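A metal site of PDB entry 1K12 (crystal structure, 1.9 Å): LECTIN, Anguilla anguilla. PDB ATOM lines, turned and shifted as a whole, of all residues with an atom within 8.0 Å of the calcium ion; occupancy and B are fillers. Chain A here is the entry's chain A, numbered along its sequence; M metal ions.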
ATOM      1  N   GLU A  32      -8.755  -5.455   0.105  1.00  0.00           N
ATOM      2  CA  GLU A  32      -9.824  -5.732   1.066  1.00  0.00           C
ATOM      3  C   GLU A  32     -11.255  -5.473   0.626  1.00  0.00           C
ATOM      4  O   GLU A  32     -11.566  -4.444   0.027  1.00  0.00           O
ATOM      5  CB  GLU A  32      -9.557  -4.976   2.368  1.00  0.00           C
ATOM      6  CG  GLU A  32      -9.091  -5.856   3.517  1.00  0.00           C
ATOM      7  CD  GLU A  32     -10.222  -6.453   4.354  1.00  0.00           C
ATOM      8  OE1 GLU A  32     -11.312  -5.862   4.433  1.00  0.00           O
ATOM      9  OE2 GLU A  32      -9.996  -7.512   4.965  1.00  0.00           O
ATOM     10  N   ALA A  33     -12.140  -6.423   0.941  1.00  0.00           N
ATOM     11  CA  ALA A  33     -13.552  -6.324   0.588  1.00  0.00           C
ATOM     12  C   ALA A  33     -14.146  -5.010   1.080  1.00  0.00           C
ATOM     13  O   ALA A  33     -15.019  -4.432   0.438  1.00  0.00           O
ATOM     14  CB  ALA A  33     -14.320  -7.507   1.171  1.00  0.00           C
ATOM     15  N   SER A  34     -13.676  -4.547   2.239  1.00  0.00           N
ATOM     16  CA  SER A  34     -14.177  -3.307   2.843  1.00  0.00           C
ATOM     17  C   SER A  34     -13.993  -2.077   1.962  1.00  0.00           C
ATOM     18  O   SER A  34     -14.715  -1.086   2.101  1.00  0.00           O
ATOM     19  CB  SER A  34     -13.502  -3.068   4.200  1.00  0.00           C
ATOM     20  OG  SER A  34     -12.107  -2.886   4.056  1.00  0.00           O
ATOM     21  N   ASN A  35     -13.037  -2.136   1.031  1.00  0.00           N
ATOM     22  CA  ASN A  35     -12.744  -1.019   0.149  1.00  0.00           C
ATOM     23  C   ASN A  35     -13.901  -0.570  -0.729  1.00  0.00           C
ATOM     24  O   ASN A  35     -13.938   0.578  -1.136  1.00  0.00           O
ATOM     25  CB  ASN A  35     -11.509  -1.331  -0.732  1.00  0.00           C
ATOM     26  CG  ASN A  35     -10.208  -1.392   0.067  1.00  0.00           C
ATOM     27  OD1 ASN A  35     -10.140  -0.911   1.205  1.00  0.00           O
ATOM     28  ND2 ASN A  35      -9.151  -1.973  -0.541  1.00  0.00           N
ATOM     29  N   ALA A  36     -14.836  -1.479  -1.032  1.00  0.00           N
ATOM     30  CA  ALA A  36     -15.981  -1.141  -1.873  1.00  0.00           C
ATOM     31  C   ALA A  36     -17.078  -0.370  -1.140  1.00  0.00           C
ATOM     32  O   ALA A  36     -18.066   0.016  -1.764  1.00  0.00           O
ATOM     33  CB  ALA A  36     -16.568  -2.387  -2.503  1.00  0.00           C
ATOM     34  N   ILE A  37     -16.933  -0.149   0.169  1.00  0.00           N
ATOM     35  CA  ILE A  37     -17.931   0.608   0.931  1.00  0.00           C
ATOM     36  C   ILE A  37     -17.296   1.614   1.884  1.00  0.00           C
ATOM     37  O   ILE A  37     -17.825   1.890   2.967  1.00  0.00           O
ATOM     38  CB  ILE A  37     -18.909  -0.328   1.727  1.00  0.00           C
ATOM     39  CG1 ILE A  37     -18.134  -1.258   2.682  1.00  0.00           C
ATOM     40  CG2 ILE A  37     -19.791  -1.124   0.750  1.00  0.00           C
ATOM     41  CD1 ILE A  37     -19.034  -2.025   3.654  1.00  0.00           C
ATOM     42  N   ASP A  38     -16.150   2.159   1.462  1.00  0.00           N
ATOM     43  CA  ASP A  38     -15.423   3.144   2.277  1.00  0.00           C
ATOM     44  C   ASP A  38     -15.729   4.599   1.903  1.00  0.00           C
ATOM     45  O   ASP A  38     -15.013   5.520   2.352  1.00  0.00           O
ATOM     46  CB  ASP A  38     -13.900   2.887   2.193  1.00  0.00           C
ATOM     47  CG  ASP A  38     -13.328   3.215   0.839  1.00  0.00           C
ATOM     48  OD1 ASP A  38     -14.108   3.441  -0.099  1.00  0.00           O
ATOM     49  OD2 ASP A  38     -12.089   3.250   0.690  1.00  0.00           O
ATOM     50  N   GLY A  39     -16.791   4.800   1.099  1.00  0.00           N
ATOM     51  CA  GLY A  39     -17.242   6.121   0.657  1.00  0.00           C
ATOM     52  C   GLY A  39     -16.310   6.854  -0.296  1.00  0.00           C
ATOM     53  O   GLY A  39     -16.360   8.079  -0.400  1.00  0.00           O
ATOM     54  N   ASN A  40     -15.476   6.117  -1.030  1.00  0.00           N
ATOM     55  CA  ASN A  40     -14.493   6.687  -1.946  1.00  0.00           C
ATOM     56  C   ASN A  40     -14.587   5.960  -3.293  1.00  0.00           C
ATOM     57  O   ASN A  40     -14.355   4.760  -3.368  1.00  0.00           O
ATOM     58  CB  ASN A  40     -13.099   6.509  -1.340  1.00  0.00           C
ATOM     59  CG  ASN A  40     -12.009   7.224  -2.126  1.00  0.00           C
ATOM     60  OD1 ASN A  40     -12.210   7.663  -3.268  1.00  0.00           O
ATOM     61  ND2 ASN A  40     -10.837   7.329  -1.516  1.00  0.00           N
ATOM     62  N   ARG A  41     -14.899   6.707  -4.355  1.00  0.00           N
ATOM     63  CA  ARG A  41     -15.017   6.116  -5.677  1.00  0.00           C
ATOM     64  C   ARG A  41     -13.716   6.034  -6.482  1.00  0.00           C
ATOM     65  O   ARG A  41     -13.729   5.594  -7.633  1.00  0.00           O
ATOM     66  CB  ARG A  41     -16.057   6.889  -6.489  1.00  0.00           C
ATOM     67  CG  ARG A  41     -17.478   6.748  -5.992  1.00  0.00           C
ATOM     68  CD  ARG A  41     -18.378   7.563  -6.881  1.00  0.00           C
ATOM     69  NE  ARG A  41     -19.787   7.402  -6.552  1.00  0.00           N
ATOM     70  CZ  ARG A  41     -20.765   8.119  -7.099  1.00  0.00           C
ATOM     71  NH1 ARG A  41     -20.477   9.050  -8.004  1.00  0.00           N
ATOM     72  NH2 ARG A  41     -22.031   7.906  -6.742  1.00  0.00           N
ATOM     73  N   ASP A  42     -12.605   6.447  -5.888  1.00  0.00           N
ATOM     74  CA  ASP A  42     -11.313   6.393  -6.577  1.00  0.00           C
ATOM     75  C   ASP A  42     -11.166   5.045  -7.281  1.00  0.00           C
ATOM     76  O   ASP A  42     -11.180   3.995  -6.624  1.00  0.00           O
ATOM     77  CB  ASP A  42     -10.173   6.600  -5.571  1.00  0.00           C
ATOM     78  CG  ASP A  42      -8.834   6.988  -6.239  1.00  0.00           C
ATOM     79  OD1 ASP A  42      -8.632   6.676  -7.442  1.00  0.00           O
ATOM     80  OD2 ASP A  42      -7.985   7.581  -5.546  1.00  0.00           O
ATOM     81  N   SER A  43     -11.024   5.075  -8.601  1.00  0.00           N
ATOM     82  CA  SER A  43     -10.905   3.845  -9.381  1.00  0.00           C
ATOM     83  C   SER A  43      -9.478   3.421  -9.734  1.00  0.00           C
ATOM     84  O   SER A  43      -9.271   2.482 -10.489  1.00  0.00           O
ATOM     85  CB  SER A  43     -11.759   3.922 -10.661  1.00  0.00           C
ATOM     86  OG  SER A  43     -11.244   4.848 -11.591  1.00  0.00           O
ATOM     87  N   GLY A  48      -5.752   2.101  -3.116  1.00  0.00           N
ATOM     88  CA  GLY A  48      -6.279   1.338  -2.000  1.00  0.00           C
ATOM     89  C   GLY A  48      -7.760   1.458  -1.687  1.00  0.00           C
ATOM     90  O   GLY A  48      -8.162   1.131  -0.574  1.00  0.00           O
ATOM     91  N   SER A  49      -8.584   1.903  -2.638  1.00  0.00           N
ATOM     92  CA  SER A  49     -10.013   2.008  -2.379  1.00  0.00           C
ATOM     93  C   SER A  49     -10.863   1.045  -3.228  1.00  0.00           C
ATOM     94  O   SER A  49     -12.056   1.246  -3.393  1.00  0.00           O
ATOM     95  CB  SER A  49     -10.487   3.447  -2.546  1.00  0.00           C
ATOM     96  OG  SER A  49     -11.699   3.666  -1.828  1.00  0.00           O
ATOM     97  N   CYS A  50     -10.243  -0.022  -3.748  1.00  0.00           N
ATOM     98  CA  CYS A  50     -10.983  -1.012  -4.537  1.00  0.00           C
ATOM     99  C   CYS A  50     -10.757  -2.415  -3.970  1.00  0.00           C
ATOM    100  O   CYS A  50      -9.710  -2.693  -3.373  1.00  0.00           O
ATOM    101  CB  CYS A  50     -10.530  -1.005  -6.016  1.00  0.00           C
ATOM    102  SG  CYS A  50     -10.485   0.605  -6.856  1.00  0.00           S
ATOM    103  N   THR A  51     -11.736  -3.289  -4.166  1.00  0.00           N
ATOM    104  CA  THR A  51     -11.618  -4.679  -3.725  1.00  0.00           C
ATOM    105  C   THR A  51     -10.994  -5.460  -4.878  1.00  0.00           C
ATOM    106  O   THR A  51     -10.920  -4.977  -6.001  1.00  0.00           O
ATOM    107  CB  THR A  51     -12.998  -5.308  -3.435  1.00  0.00           C
ATOM    108  OG1 THR A  51     -13.687  -5.532  -4.676  1.00  0.00           O
ATOM    109  CG2 THR A  51     -13.831  -4.397  -2.547  1.00  0.00           C
ATOM    110  N   THR A  77     -18.801   1.339  -9.183  1.00  0.00           N
ATOM    111  CA  THR A  77     -17.673   2.040  -9.794  1.00  0.00           C
ATOM    112  C   THR A  77     -16.700   0.939 -10.185  1.00  0.00           C
ATOM    113  O   THR A  77     -16.190   0.191  -9.351  1.00  0.00           O
ATOM    114  CB  THR A  77     -16.967   3.029  -8.847  1.00  0.00           C
ATOM    115  OG1 THR A  77     -17.881   4.087  -8.493  1.00  0.00           O
ATOM    116  CG2 THR A  77     -15.728   3.634  -9.547  1.00  0.00           C
ATOM    117  N   LEU A 145     -14.150  -4.228  -7.484  1.00  0.00           N
ATOM    118  CA  LEU A 145     -15.152  -3.160  -7.340  1.00  0.00           C
ATOM    119  C   LEU A 145     -14.534  -1.990  -6.581  1.00  0.00           C
ATOM    120  O   LEU A 145     -13.985  -2.176  -5.496  1.00  0.00           O
ATOM    121  CB  LEU A 145     -16.341  -3.704  -6.549  1.00  0.00           C
ATOM    122  CG  LEU A 145     -17.084  -4.863  -7.212  1.00  0.00           C
ATOM    123  CD1 LEU A 145     -17.865  -5.661  -6.152  1.00  0.00           C
ATOM    124  CD2 LEU A 145     -18.015  -4.306  -8.310  1.00  0.00           C
ATOM    125  N   CYS A 146     -14.619  -0.781  -7.120  1.00  0.00           N
ATOM    126  CA  CYS A 146     -14.036   0.358  -6.414  1.00  0.00           C
ATOM    127  C   CYS A 146     -15.043   1.007  -5.484  1.00  0.00           C
ATOM    128  O   CYS A 146     -14.675   1.735  -4.585  1.00  0.00           O
ATOM    129  CB  CYS A 146     -13.431   1.358  -7.381  1.00  0.00           C
ATOM    130  SG  CYS A 146     -12.002   0.593  -8.223  1.00  0.00           S
ATOM    131  N   GLU A 147     -16.319   0.728  -5.701  1.00  0.00           N
ATOM    132  CA  GLU A 147     -17.349   1.229  -4.811  1.00  0.00           C
ATOM    133  C   GLU A 147     -18.701   0.646  -5.198  1.00  0.00           C
ATOM    134  O   GLU A 147     -19.035   0.570  -6.371  1.00  0.00           O
ATOM    135  CB  GLU A 147     -17.411   2.776  -4.802  1.00  0.00           C
ATOM    136  CG  GLU A 147     -18.207   3.385  -3.621  1.00  0.00           C
ATOM    137  CD  GLU A 147     -17.563   3.161  -2.234  1.00  0.00           C
ATOM    138  OE1 GLU A 147     -16.349   2.835  -2.160  1.00  0.00           O
ATOM    139  OE2 GLU A 147     -18.272   3.331  -1.216  1.00  0.00           O
ATOM    140  N   VAL A 148     -19.450   0.207  -4.187  1.00  0.00           N
ATOM    141  CA  VAL A 148     -20.779  -0.347  -4.362  1.00  0.00           C
ATOM    142  C   VAL A 148     -21.661   0.458  -3.399  1.00  0.00           C
ATOM    143  O   VAL A 148     -21.489   0.440  -2.180  1.00  0.00           O
ATOM    144  CB  VAL A 148     -20.837  -1.844  -4.004  1.00  0.00           C
ATOM    145  CG1 VAL A 148     -22.263  -2.365  -4.138  1.00  0.00           C
ATOM    146  CG2 VAL A 148     -19.912  -2.637  -4.905  1.00  0.00           C
ATOM    147  N   GLU A 149     -22.604   1.195  -3.986  1.00  0.00           N
ATOM    148  CA  GLU A 149     -23.511   2.025  -3.231  1.00  0.00           C
ATOM    149  C   GLU A 149     -24.917   1.444  -3.375  1.00  0.00           C
ATOM    150  O   GLU A 149     -25.368   1.167  -4.478  1.00  0.00           O
ATOM    151  CB  GLU A 149     -23.441   3.441  -3.784  1.00  0.00           C
ATOM    152  CG  GLU A 149     -22.093   4.107  -3.550  1.00  0.00           C
ATOM    153  CD  GLU A 149     -21.868   5.330  -4.410  1.00  0.00           C
ATOM    154  OE1 GLU A 149     -22.821   6.087  -4.669  1.00  0.00           O
ATOM    155  OE2 GLU A 149     -20.721   5.551  -4.836  1.00  0.00           O
HETATM  156 CA    CA M   1     -13.941   2.579  -2.495  1.00  0.00          CA
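The side-chain amide oxygen (OD1) of Asn 40 lies within hydrogen-bond range of the backbone NH (N) of Asp 42, at 2.9 Å.
The side-chain carboxylate (OE2) of Glu 147 sits at hydrogen-bond distance from the backbone NH (N) of Gly 39, at 3.1 Å.
The backbone carbonyl oxygen of Glu 147 lies within hydrogen-bond range of the backbone NH of Thr 77 (2.9 Å).
The side-chain amide nitrogen of Asn 35 is in hydrogen-bond range of the backbone carbonyl oxygen of Cys 50 (3.0 Å).
The side-chain amide nitrogen of Asn 35 sits at hydrogen-bond distance from the backbone carbonyl oxygen of Gly 48, 3.3 Å away.
The backbone carbonyl oxygen of Thr 77 sits at hydrogen-bond distance from the backbone NH of Cys 146, 2.9 Å away.
The side-chain sulfur (SG) of Cys 50 forms a disulfide with the side-chain sulfur (SG) of Cys 146 (2.0 Å).
Of the 22 residues printed, 6 come within 4 Å of the calcium ion.
The nearest printed residue that does not touch the calcium ion is Ala 36 (4.3 Å).
The calcium ion is bound by the backbone carbonyl oxygen (O) of Cys 146, the backbone carbonyl oxygen (O) of Asn 40, the backbone carbonyl oxygen (O) of Asn 35, the side-chain carboxylate (OE1) of Glu 147, the backbone carbonyl oxygen (O) of Ser 49, the side-chain carboxylate (OD1) of Asp 38 and the side-chain hydroxyl (OG) of Ser 49.
The calcium ion has seven donor atoms within binding distance.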
